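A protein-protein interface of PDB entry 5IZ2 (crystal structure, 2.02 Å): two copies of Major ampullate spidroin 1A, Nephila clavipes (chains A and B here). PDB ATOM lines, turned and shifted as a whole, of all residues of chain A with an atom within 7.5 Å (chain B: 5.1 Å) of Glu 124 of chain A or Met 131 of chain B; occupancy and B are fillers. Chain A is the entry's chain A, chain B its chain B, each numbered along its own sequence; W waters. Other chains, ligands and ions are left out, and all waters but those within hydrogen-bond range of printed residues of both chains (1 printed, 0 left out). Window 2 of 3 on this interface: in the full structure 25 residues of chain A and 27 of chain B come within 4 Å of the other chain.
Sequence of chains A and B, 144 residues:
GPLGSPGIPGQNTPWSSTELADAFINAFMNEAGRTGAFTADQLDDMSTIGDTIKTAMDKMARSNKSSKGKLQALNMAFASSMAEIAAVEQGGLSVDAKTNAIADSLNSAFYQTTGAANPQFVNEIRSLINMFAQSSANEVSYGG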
ATOM      1  N   GLN A  72     -17.610 -43.053  -4.093  1.00  0.00           N
ATOM      2  CA  GLN A  72     -17.997 -41.808  -3.444  1.00  0.00           C
ATOM      3  C   GLN A  72     -16.778 -40.906  -3.218  1.00  0.00           C
ATOM      4  O   GLN A  72     -16.846 -39.695  -3.403  1.00  0.00           O
ATOM      5  CB  GLN A  72     -18.731 -42.078  -2.131  1.00  0.00           C
ATOM      6  CG  GLN A  72     -19.280 -40.810  -1.518  1.00  0.00           C
ATOM      7  CD  GLN A  72     -20.198 -41.063  -0.347  1.00  0.00           C
ATOM      8  OE1 GLN A  72     -20.356 -42.194   0.104  1.00  0.00           O
ATOM      9  NE2 GLN A  72     -20.828 -40.005   0.140  1.00  0.00           N
ATOM     10  N   MET A  76     -15.894 -37.216  -4.903  1.00  0.00           N
ATOM     11  CA  MET A  76     -15.454 -36.021  -4.186  1.00  0.00           C
ATOM     12  C   MET A  76     -14.133 -35.486  -4.740  1.00  0.00           C
ATOM     13  O   MET A  76     -13.933 -34.274  -4.796  1.00  0.00           O
ATOM     14  CB  MET A  76     -15.324 -36.302  -2.685  1.00  0.00           C
ATOM     15  CG  MET A  76     -14.889 -35.095  -1.855  1.00  0.00           C
ATOM     16  SD  MET A  76     -15.993 -33.673  -2.050  1.00  0.00           S
ATOM     17  CE  MET A  76     -17.554 -34.367  -1.517  1.00  0.00           C
ATOM     18  N   LEU A 106     -22.863 -29.260 -11.459  1.00  0.00           N
ATOM     19  CA  LEU A 106     -23.141 -30.313 -10.488  1.00  0.00           C
ATOM     20  C   LEU A 106     -24.626 -30.678 -10.464  1.00  0.00           C
ATOM     21  O   LEU A 106     -24.979 -31.857 -10.470  1.00  0.00           O
ATOM     22  CB  LEU A 106     -22.681 -29.886  -9.091  1.00  0.00           C
ATOM     23  CG  LEU A 106     -21.169 -29.880  -8.866  1.00  0.00           C
ATOM     24  CD1 LEU A 106     -20.822 -29.269  -7.512  1.00  0.00           C
ATOM     25  CD2 LEU A 106     -20.600 -31.284  -8.982  1.00  0.00           C
ATOM     26  N   ASN A 118     -29.111 -32.026  -6.292  1.00  0.00           N
ATOM     27  CA  ASN A 118     -28.639 -32.292  -4.939  1.00  0.00           C
ATOM     28  C   ASN A 118     -28.072 -31.018  -4.334  1.00  0.00           C
ATOM     29  O   ASN A 118     -26.861 -30.803  -4.353  1.00  0.00           O
ATOM     30  CB  ASN A 118     -27.590 -33.410  -4.947  1.00  0.00           C
ATOM     31  CG  ASN A 118     -27.281 -33.946  -3.557  1.00  0.00           C
ATOM     32  OD1 ASN A 118     -27.532 -33.290  -2.549  1.00  0.00           O
ATOM     33  ND2 ASN A 118     -26.726 -35.153  -3.503  1.00  0.00           N
ATOM     34  N   PRO A 119     -28.960 -30.149  -3.822  1.00  0.00           N
ATOM     35  CA  PRO A 119     -28.562 -28.852  -3.261  1.00  0.00           C
ATOM     36  C   PRO A 119     -27.648 -29.003  -2.044  1.00  0.00           C
ATOM     37  O   PRO A 119     -26.781 -28.155  -1.820  1.00  0.00           O
ATOM     38  CB  PRO A 119     -29.898 -28.205  -2.874  1.00  0.00           C
ATOM     39  CG  PRO A 119     -30.857 -29.331  -2.761  1.00  0.00           C
ATOM     40  CD  PRO A 119     -30.417 -30.353  -3.761  1.00  0.00           C
ATOM     41  N   GLN A 120     -27.847 -30.065  -1.269  1.00  0.00           N
ATOM     42  CA  GLN A 120     -27.000 -30.342  -0.111  1.00  0.00           C
ATOM     43  C   GLN A 120     -25.542 -30.538  -0.531  1.00  0.00           C
ATOM     44  O   GLN A 120     -24.635 -29.927   0.034  1.00  0.00           O
ATOM     45  CB  GLN A 120     -27.508 -31.573   0.640  1.00  0.00           C
ATOM     46  CG  GLN A 120     -26.562 -32.100   1.705  1.00  0.00           C
ATOM     47  CD  GLN A 120     -25.992 -33.464   1.354  1.00  0.00           C
ATOM     48  OE1 GLN A 120     -26.356 -34.059   0.336  1.00  0.00           O
ATOM     49  NE2 GLN A 120     -25.096 -33.968   2.197  1.00  0.00           N
ATOM     50  N   PHE A 121     -25.331 -31.378  -1.539  1.00  0.00           N
ATOM     51  CA  PHE A 121     -23.992 -31.646  -2.051  1.00  0.00           C
ATOM     52  C   PHE A 121     -23.343 -30.369  -2.572  1.00  0.00           C
ATOM     53  O   PHE A 121     -22.187 -30.079  -2.269  1.00  0.00           O
ATOM     54  CB  PHE A 121     -24.045 -32.698  -3.159  1.00  0.00           C
ATOM     55  CG  PHE A 121     -22.696 -33.182  -3.605  1.00  0.00           C
ATOM     56  CD1 PHE A 121     -22.122 -34.303  -3.027  1.00  0.00           C
ATOM     57  CD2 PHE A 121     -22.000 -32.518  -4.608  1.00  0.00           C
ATOM     58  CE1 PHE A 121     -20.876 -34.755  -3.440  1.00  0.00           C
ATOM     59  CE2 PHE A 121     -20.759 -32.967  -5.026  1.00  0.00           C
ATOM     60  CZ  PHE A 121     -20.197 -34.086  -4.440  1.00  0.00           C
ATOM     61  N   VAL A 122     -24.104 -29.606  -3.346  1.00  0.00           N
ATOM     62  CA  VAL A 122     -23.601 -28.381  -3.954  1.00  0.00           C
ATOM     63  C   VAL A 122     -23.183 -27.370  -2.883  1.00  0.00           C
ATOM     64  O   VAL A 122     -22.147 -26.715  -3.003  1.00  0.00           O
ATOM     65  CB  VAL A 122     -24.658 -27.756  -4.884  1.00  0.00           C
ATOM     66  CG1 VAL A 122     -24.227 -26.375  -5.338  1.00  0.00           C
ATOM     67  CG2 VAL A 122     -24.908 -28.667  -6.079  1.00  0.00           C
ATOM     68  N   ASN A 123     -23.989 -27.252  -1.833  1.00  0.00           N
ATOM     69  CA  ASN A 123     -23.654 -26.357  -0.734  1.00  0.00           C
ATOM     70  C   ASN A 123     -22.352 -26.752  -0.041  1.00  0.00           C
ATOM     71  O   ASN A 123     -21.613 -25.885   0.430  1.00  0.00           O
ATOM     72  CB  ASN A 123     -24.795 -26.306   0.283  1.00  0.00           C
ATOM     73  CG  ASN A 123     -25.981 -25.513  -0.219  1.00  0.00           C
ATOM     74  OD1 ASN A 123     -25.834 -24.622  -1.057  1.00  0.00           O
ATOM     75  ND2 ASN A 123     -27.164 -25.819   0.300  1.00  0.00           N
ATOM     76  N   GLU A 124     -22.065 -28.051   0.017  1.00  0.00           N
ATOM     77  CA  GLU A 124     -20.781 -28.508   0.548  1.00  0.00           C
ATOM     78  C   GLU A 124     -19.623 -28.072  -0.342  1.00  0.00           C
ATOM     79  O   GLU A 124     -18.578 -27.643   0.155  1.00  0.00           O
ATOM     80  CB  GLU A 124     -20.743 -30.029   0.712  1.00  0.00           C
ATOM     81  CG  GLU A 124     -21.458 -30.555   1.943  1.00  0.00           C
ATOM     82  CD  GLU A 124     -21.489 -32.073   1.990  1.00  0.00           C
ATOM     83  OE1 GLU A 124     -21.073 -32.710   0.999  1.00  0.00           O
ATOM     84  OE2 GLU A 124     -21.908 -32.628   3.025  1.00  0.00           O
ATOM     85  N   ILE A 125     -19.813 -28.180  -1.654  1.00  0.00           N
ATOM     86  CA  ILE A 125     -18.786 -27.769  -2.604  1.00  0.00           C
ATOM     87  C   ILE A 125     -18.534 -26.266  -2.520  1.00  0.00           C
ATOM     88  O   ILE A 125     -17.390 -25.817  -2.600  1.00  0.00           O
ATOM     89  CB  ILE A 125     -19.171 -28.130  -4.048  1.00  0.00           C
ATOM     90  CG1 ILE A 125     -19.430 -29.635  -4.169  1.00  0.00           C
ATOM     91  CG2 ILE A 125     -18.072 -27.699  -5.016  1.00  0.00           C
ATOM     92  CD1 ILE A 125     -18.302 -30.486  -3.643  1.00  0.00           C
ATOM     93  N   ARG A 126     -19.604 -25.498  -2.342  1.00  0.00           N
ATOM     94  CA  ARG A 126     -19.483 -24.061  -2.130  1.00  0.00           C
ATOM     95  C   ARG A 126     -18.657 -23.776  -0.881  1.00  0.00           C
ATOM     96  O   ARG A 126     -17.779 -22.912  -0.888  1.00  0.00           O
ATOM     97  CB  ARG A 126     -20.859 -23.408  -2.000  1.00  0.00           C
ATOM     98  CG  ARG A 126     -21.724 -23.463  -3.244  1.00  0.00           C
ATOM     99  CD  ARG A 126     -22.991 -22.645  -3.022  1.00  0.00           C
ATOM    100  NE  ARG A 126     -23.971 -22.809  -4.093  1.00  0.00           N
ATOM    101  CZ  ARG A 126     -24.014 -22.059  -5.188  1.00  0.00           C
ATOM    102  NH1 ARG A 126     -23.124 -21.090  -5.367  1.00  0.00           N
ATOM    103  NH2 ARG A 126     -24.945 -22.276  -6.107  1.00  0.00           N
ATOM    104  N   SER A 127     -18.947 -24.513   0.188  1.00  0.00           N
ATOM    105  CA  SER A 127     -18.228 -24.363   1.450  1.00  0.00           C
ATOM    106  C   SER A 127     -16.768 -24.780   1.298  1.00  0.00           C
ATOM    107  O   SER A 127     -15.876 -24.196   1.919  1.00  0.00           O
ATOM    108  CB  SER A 127     -18.896 -25.189   2.551  1.00  0.00           C
ATOM    109  OG  SER A 127     -20.215 -24.740   2.798  1.00  0.00           O
ATOM    110  N   LEU A 128     -16.528 -25.792   0.470  1.00  0.00           N
ATOM    111  CA  LEU A 128     -15.176 -26.294   0.268  1.00  0.00           C
ATOM    112  C   LEU A 128     -14.328 -25.225  -0.405  1.00  0.00           C
ATOM    113  O   LEU A 128     -13.183 -24.989  -0.015  1.00  0.00           O
ATOM    114  CB  LEU A 128     -15.195 -27.578  -0.573  1.00  0.00           C
ATOM    115  CG  LEU A 128     -13.889 -28.352  -0.782  1.00  0.00           C
ATOM    116  CD1 LEU A 128     -14.163 -29.845  -0.875  1.00  0.00           C
ATOM    117  CD2 LEU A 128     -13.174 -27.881  -2.042  1.00  0.00           C
ATOM    118  N   ILE A 129     -14.918 -24.564  -1.397  1.00  0.00           N
ATOM    119  CA  ILE A 129     -14.251 -23.506  -2.145  1.00  0.00           C
ATOM    120  C   ILE A 129     -13.855 -22.345  -1.229  1.00  0.00           C
ATOM    121  O   ILE A 129     -12.743 -21.820  -1.317  1.00  0.00           O
ATOM    122  CB  ILE A 129     -15.151 -22.995  -3.295  1.00  0.00           C
ATOM    123  CG1 ILE A 129     -15.294 -24.077  -4.369  1.00  0.00           C
ATOM    124  CG2 ILE A 129     -14.597 -21.714  -3.899  1.00  0.00           C
ATOM    125  CD1 ILE A 129     -16.335 -23.766  -5.425  1.00  0.00           C
ATOM    126  N   ASN A 130     -14.767 -21.955  -0.347  1.00  0.00           N
ATOM    127  CA  ASN A 130     -14.505 -20.875   0.599  1.00  0.00           C
ATOM    128  C   ASN A 130     -13.369 -21.167   1.582  1.00  0.00           C
ATOM    129  O   ASN A 130     -12.576 -20.281   1.890  1.00  0.00           O
ATOM    130  CB  ASN A 130     -15.782 -20.539   1.368  1.00  0.00           C
ATOM    131  CG  ASN A 130     -16.826 -19.875   0.490  1.00  0.00           C
ATOM    132  OD1 ASN A 130     -16.494 -19.251  -0.518  1.00  0.00           O
ATOM    133  ND2 ASN A 130     -18.094 -20.009   0.866  1.00  0.00           N
ATOM    134  N   MET A 131     -13.294 -22.399   2.079  1.00  0.00           N
ATOM    135  CA  MET A 131     -12.243 -22.769   3.028  1.00  0.00           C
ATOM    136  C   MET A 131     -10.843 -22.681   2.427  1.00  0.00           C
ATOM    137  O   MET A 131      -9.924 -22.140   3.041  1.00  0.00           O
ATOM    138  CB  MET A 131     -12.480 -24.183   3.561  1.00  0.00           C
ATOM    139  CG  MET A 131     -13.717 -24.310   4.428  1.00  0.00           C
ATOM    140  SD  MET A 131     -13.834 -25.922   5.220  1.00  0.00           S
ATOM    141  CE  MET A 131     -15.336 -25.721   6.177  1.00  0.00           C
ATOM    142  N   SER B 127     -11.377 -28.606   9.369  1.00  0.00           N
ATOM    143  CA  SER B 127     -12.687 -27.975   9.217  1.00  0.00           C
ATOM    144  C   SER B 127     -13.525 -28.697   8.172  1.00  0.00           C
ATOM    145  O   SER B 127     -14.747 -28.811   8.294  1.00  0.00           O
ATOM    146  CB  SER B 127     -12.536 -26.503   8.830  1.00  0.00           C
ATOM    147  OG  SER B 127     -11.877 -25.777   9.851  1.00  0.00           O
ATOM    148  N   LEU B 128     -12.855 -29.180   7.136  1.00  0.00           N
ATOM    149  CA  LEU B 128     -13.535 -29.851   6.041  1.00  0.00           C
ATOM    150  C   LEU B 128     -14.134 -31.169   6.538  1.00  0.00           C
ATOM    151  O   LEU B 128     -15.251 -31.533   6.170  1.00  0.00           O
ATOM    152  CB  LEU B 128     -12.563 -30.071   4.883  1.00  0.00           C
ATOM    153  CG  LEU B 128     -13.127 -30.557   3.555  1.00  0.00           C
ATOM    154  CD1 LEU B 128     -14.164 -29.569   3.062  1.00  0.00           C
ATOM    155  CD2 LEU B 128     -12.005 -30.690   2.537  1.00  0.00           C
ATOM    156  N   ILE B 129     -13.382 -31.883   7.374  1.00  0.00           N
ATOM    157  CA  ILE B 129     -13.852 -33.139   7.945  1.00  0.00           C
ATOM    158  C   ILE B 129     -15.095 -32.912   8.795  1.00  0.00           C
ATOM    159  O   ILE B 129     -16.081 -33.642   8.681  1.00  0.00           O
ATOM    160  CB  ILE B 129     -12.771 -33.816   8.800  1.00  0.00           C
ATOM    161  CG1 ILE B 129     -11.639 -34.339   7.907  1.00  0.00           C
ATOM    162  CG2 ILE B 129     -13.365 -34.966   9.613  1.00  0.00           C
ATOM    163  CD1 ILE B 129     -10.427 -34.824   8.689  1.00  0.00           C
ATOM    164  N   ASN B 130     -15.054 -31.877   9.627  1.00  0.00           N
ATOM    165  CA  ASN B 130     -16.192 -31.544  10.473  1.00  0.00           C
ATOM    166  C   ASN B 130     -17.412 -31.196   9.632  1.00  0.00           C
ATOM    167  O   ASN B 130     -18.538 -31.581   9.954  1.00  0.00           O
ATOM    168  CB  ASN B 130     -15.850 -30.381  11.401  1.00  0.00           C
ATOM    169  CG  ASN B 130     -17.047 -29.914  12.212  1.00  0.00           C
ATOM    170  OD1 ASN B 130     -17.687 -28.916  11.879  1.00  0.00           O
ATOM    171  ND2 ASN B 130     -17.358 -30.643  13.276  1.00  0.00           N
ATOM    172  N   MET B 131     -17.165 -30.469   8.549  1.00  0.00           N
ATOM    173  CA  MET B 131     -18.204 -30.043   7.625  1.00  0.00           C
ATOM    174  C   MET B 131     -18.871 -31.250   6.968  1.00  0.00           C
ATOM    175  O   MET B 131     -20.097 -31.318   6.881  1.00  0.00           O
ATOM    176  CB  MET B 131     -17.609 -29.106   6.573  1.00  0.00           C
ATOM    177  CG  MET B 131     -18.619 -28.259   5.836  1.00  0.00           C
ATOM    178  SD  MET B 131     -19.142 -29.029   4.307  1.00  0.00           S
ATOM    179  CE  MET B 131     -17.618 -29.006   3.373  1.00  0.00           C
ATOM    180  N   PHE B 132     -18.059 -32.206   6.519  1.00  0.00           N
ATOM    181  CA  PHE B 132     -18.575 -33.406   5.875  1.00  0.00           C
ATOM    182  C   PHE B 132     -19.310 -34.266   6.899  1.00  0.00           C
ATOM    183  O   PHE B 132     -20.315 -34.908   6.582  1.00  0.00           O
ATOM    184  CB  PHE B 132     -17.445 -34.219   5.237  1.00  0.00           C
ATOM    185  CG  PHE B 132     -16.930 -33.646   3.948  1.00  0.00           C
ATOM    186  CD1 PHE B 132     -17.760 -32.922   3.112  1.00  0.00           C
ATOM    187  CD2 PHE B 132     -15.615 -33.857   3.562  1.00  0.00           C
ATOM    188  CE1 PHE B 132     -17.287 -32.405   1.921  1.00  0.00           C
ATOM    189  CE2 PHE B 132     -15.134 -33.344   2.367  1.00  0.00           C
ATOM    190  CZ  PHE B 132     -15.973 -32.615   1.545  1.00  0.00           C
ATOM    191  N   ALA B 133     -18.804 -34.268   8.130  1.00  0.00           N
ATOM    192  CA  ALA B 133     -19.383 -35.072   9.206  1.00  0.00           C
ATOM    193  C   ALA B 133     -20.785 -34.596   9.593  1.00  0.00           C
ATOM    194  O   ALA B 133     -21.613 -35.391  10.040  1.00  0.00           O
ATOM    195  CB  ALA B 133     -18.469 -35.060  10.424  1.00  0.00           C
ATOM    196  N   GLN B 134     -21.041 -33.299   9.430  1.00  0.00           N
ATOM    197  CA  GLN B 134     -22.344 -32.721   9.757  1.00  0.00           C
ATOM    198  C   GLN B 134     -23.453 -33.344   8.920  1.00  0.00           C
ATOM    199  O   GLN B 134     -24.541 -33.621   9.422  1.00  0.00           O
ATOM    200  CB  GLN B 134     -22.329 -31.206   9.553  1.00  0.00           C
ATOM    201  CG  GLN B 134     -21.630 -30.432  10.654  1.00  0.00           C
ATOM    202  CD  GLN B 134     -22.464 -30.332  11.917  1.00  0.00           C
ATOM    203  OE1 GLN B 134     -23.670 -30.579  11.901  1.00  0.00           O
ATOM    204  NE2 GLN B 134     -21.822 -29.965  13.021  1.00  0.00           N
ATOM    205  N   SER B 135     -23.164 -33.565   7.641  1.00  0.00           N
ATOM    206  CA  SER B 135     -24.134 -34.139   6.717  1.00  0.00           C
ATOM    207  C   SER B 135     -24.132 -35.664   6.776  1.00  0.00           C
ATOM    208  O   SER B 135     -23.912 -36.332   5.764  1.00  0.00           O
ATOM    209  CB  SER B 135     -23.845 -33.673   5.292  1.00  0.00           C
ATOM    210  OG  SER B 135     -23.582 -32.280   5.255  1.00  0.00           O
HETATM  211  O   HOH W   1     -21.898 -26.845   3.820  1.00  0.00           O
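OE2 of Glu 124 of chain A is in hydrogen-bond range of OG of Ser 135 of chain B.
OE1 of Gln 120 of chain A sits close to OD1 of Asn 118 of chain A (3.2 Å).
Among the printed residues, merely in contact across the chains: Met 76 of chain A with Phe 132 of chain B, Gln 120 of chain A with Ser 135 of chain B, Glu 124 of chain A with Met 131 of chain B, Glu 124 of chain A with Phe 132 of chain B, Leu 128 of chain A with Leu 128 of chain B, Met 131 of chain A with Ser 127 of chain B and Met 131 of chain A with Leu 128 of chain B.
Of the printed residues of chain B, Gln 120 of chain A touches Ser 135 (3.4 Å).
Of chain B, only Met 131 (3.6 Å), Phe 132 (3.9 Å) and Ser 135 (2.8 Å) come within 4 Å of Glu 124 of chain A.
Of the printed residues of chain B, Met 131 of chain A touches Ser 127 (3.8 Å) and Leu 128 (3.9 Å).
Of the printed residues of chain A, Ser 127 of chain B touches Met 131 (3.8 Å).
Printed residues of chain A within 4 Å of Leu 128 of chain B: Leu 128 (3.9 Å) and Met 131 (3.9 Å).
Met 131 of chain B touches just one residue of chain A: Glu 124.
Of the printed residues of chain A, Ser 135 of chain B touches Gln 120 and Glu 124.
Printed residues of chain A that touch a printed residue of chain B: Met 76, Gln 120, Glu 124, Leu 128 and Met 131.
Hydrophobic or aromatic side chains of chain A within 4 Å of the printed part of chain B: Met 76, Leu 128 and Met 131.
Among the printed residues, no Asp or Glu carboxylate lies within 4 Å of a Lys or Arg side-chain nitrogen of the other chain.
Leu 128 of chain B touches its own counterpart, Leu 128 of chain A.
Met 131 of chain A touches Ser 127 of chain B, but with the chains exchanged Ser 127 of chain A does not touch Met 131 of chain B (4.1 Å).
Met 131 of chain A touches Leu 128 of chain B, but with the chains exchanged Leu 128 of chain A does not touch Met 131 of chain B (4.5 Å).
Positions printed for both chains: 127, 128, 129, 130 and 131.
Of the 8 pairs that touch across the chains among the printed residues, 1 has its exchanged pair printed and touching as well.
Water W1 bridges the side-chain hydroxyl of Ser 127 of chain A (2.9 Å) and the side-chain sulfur of Met 131 of chain B (3.6 Å).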
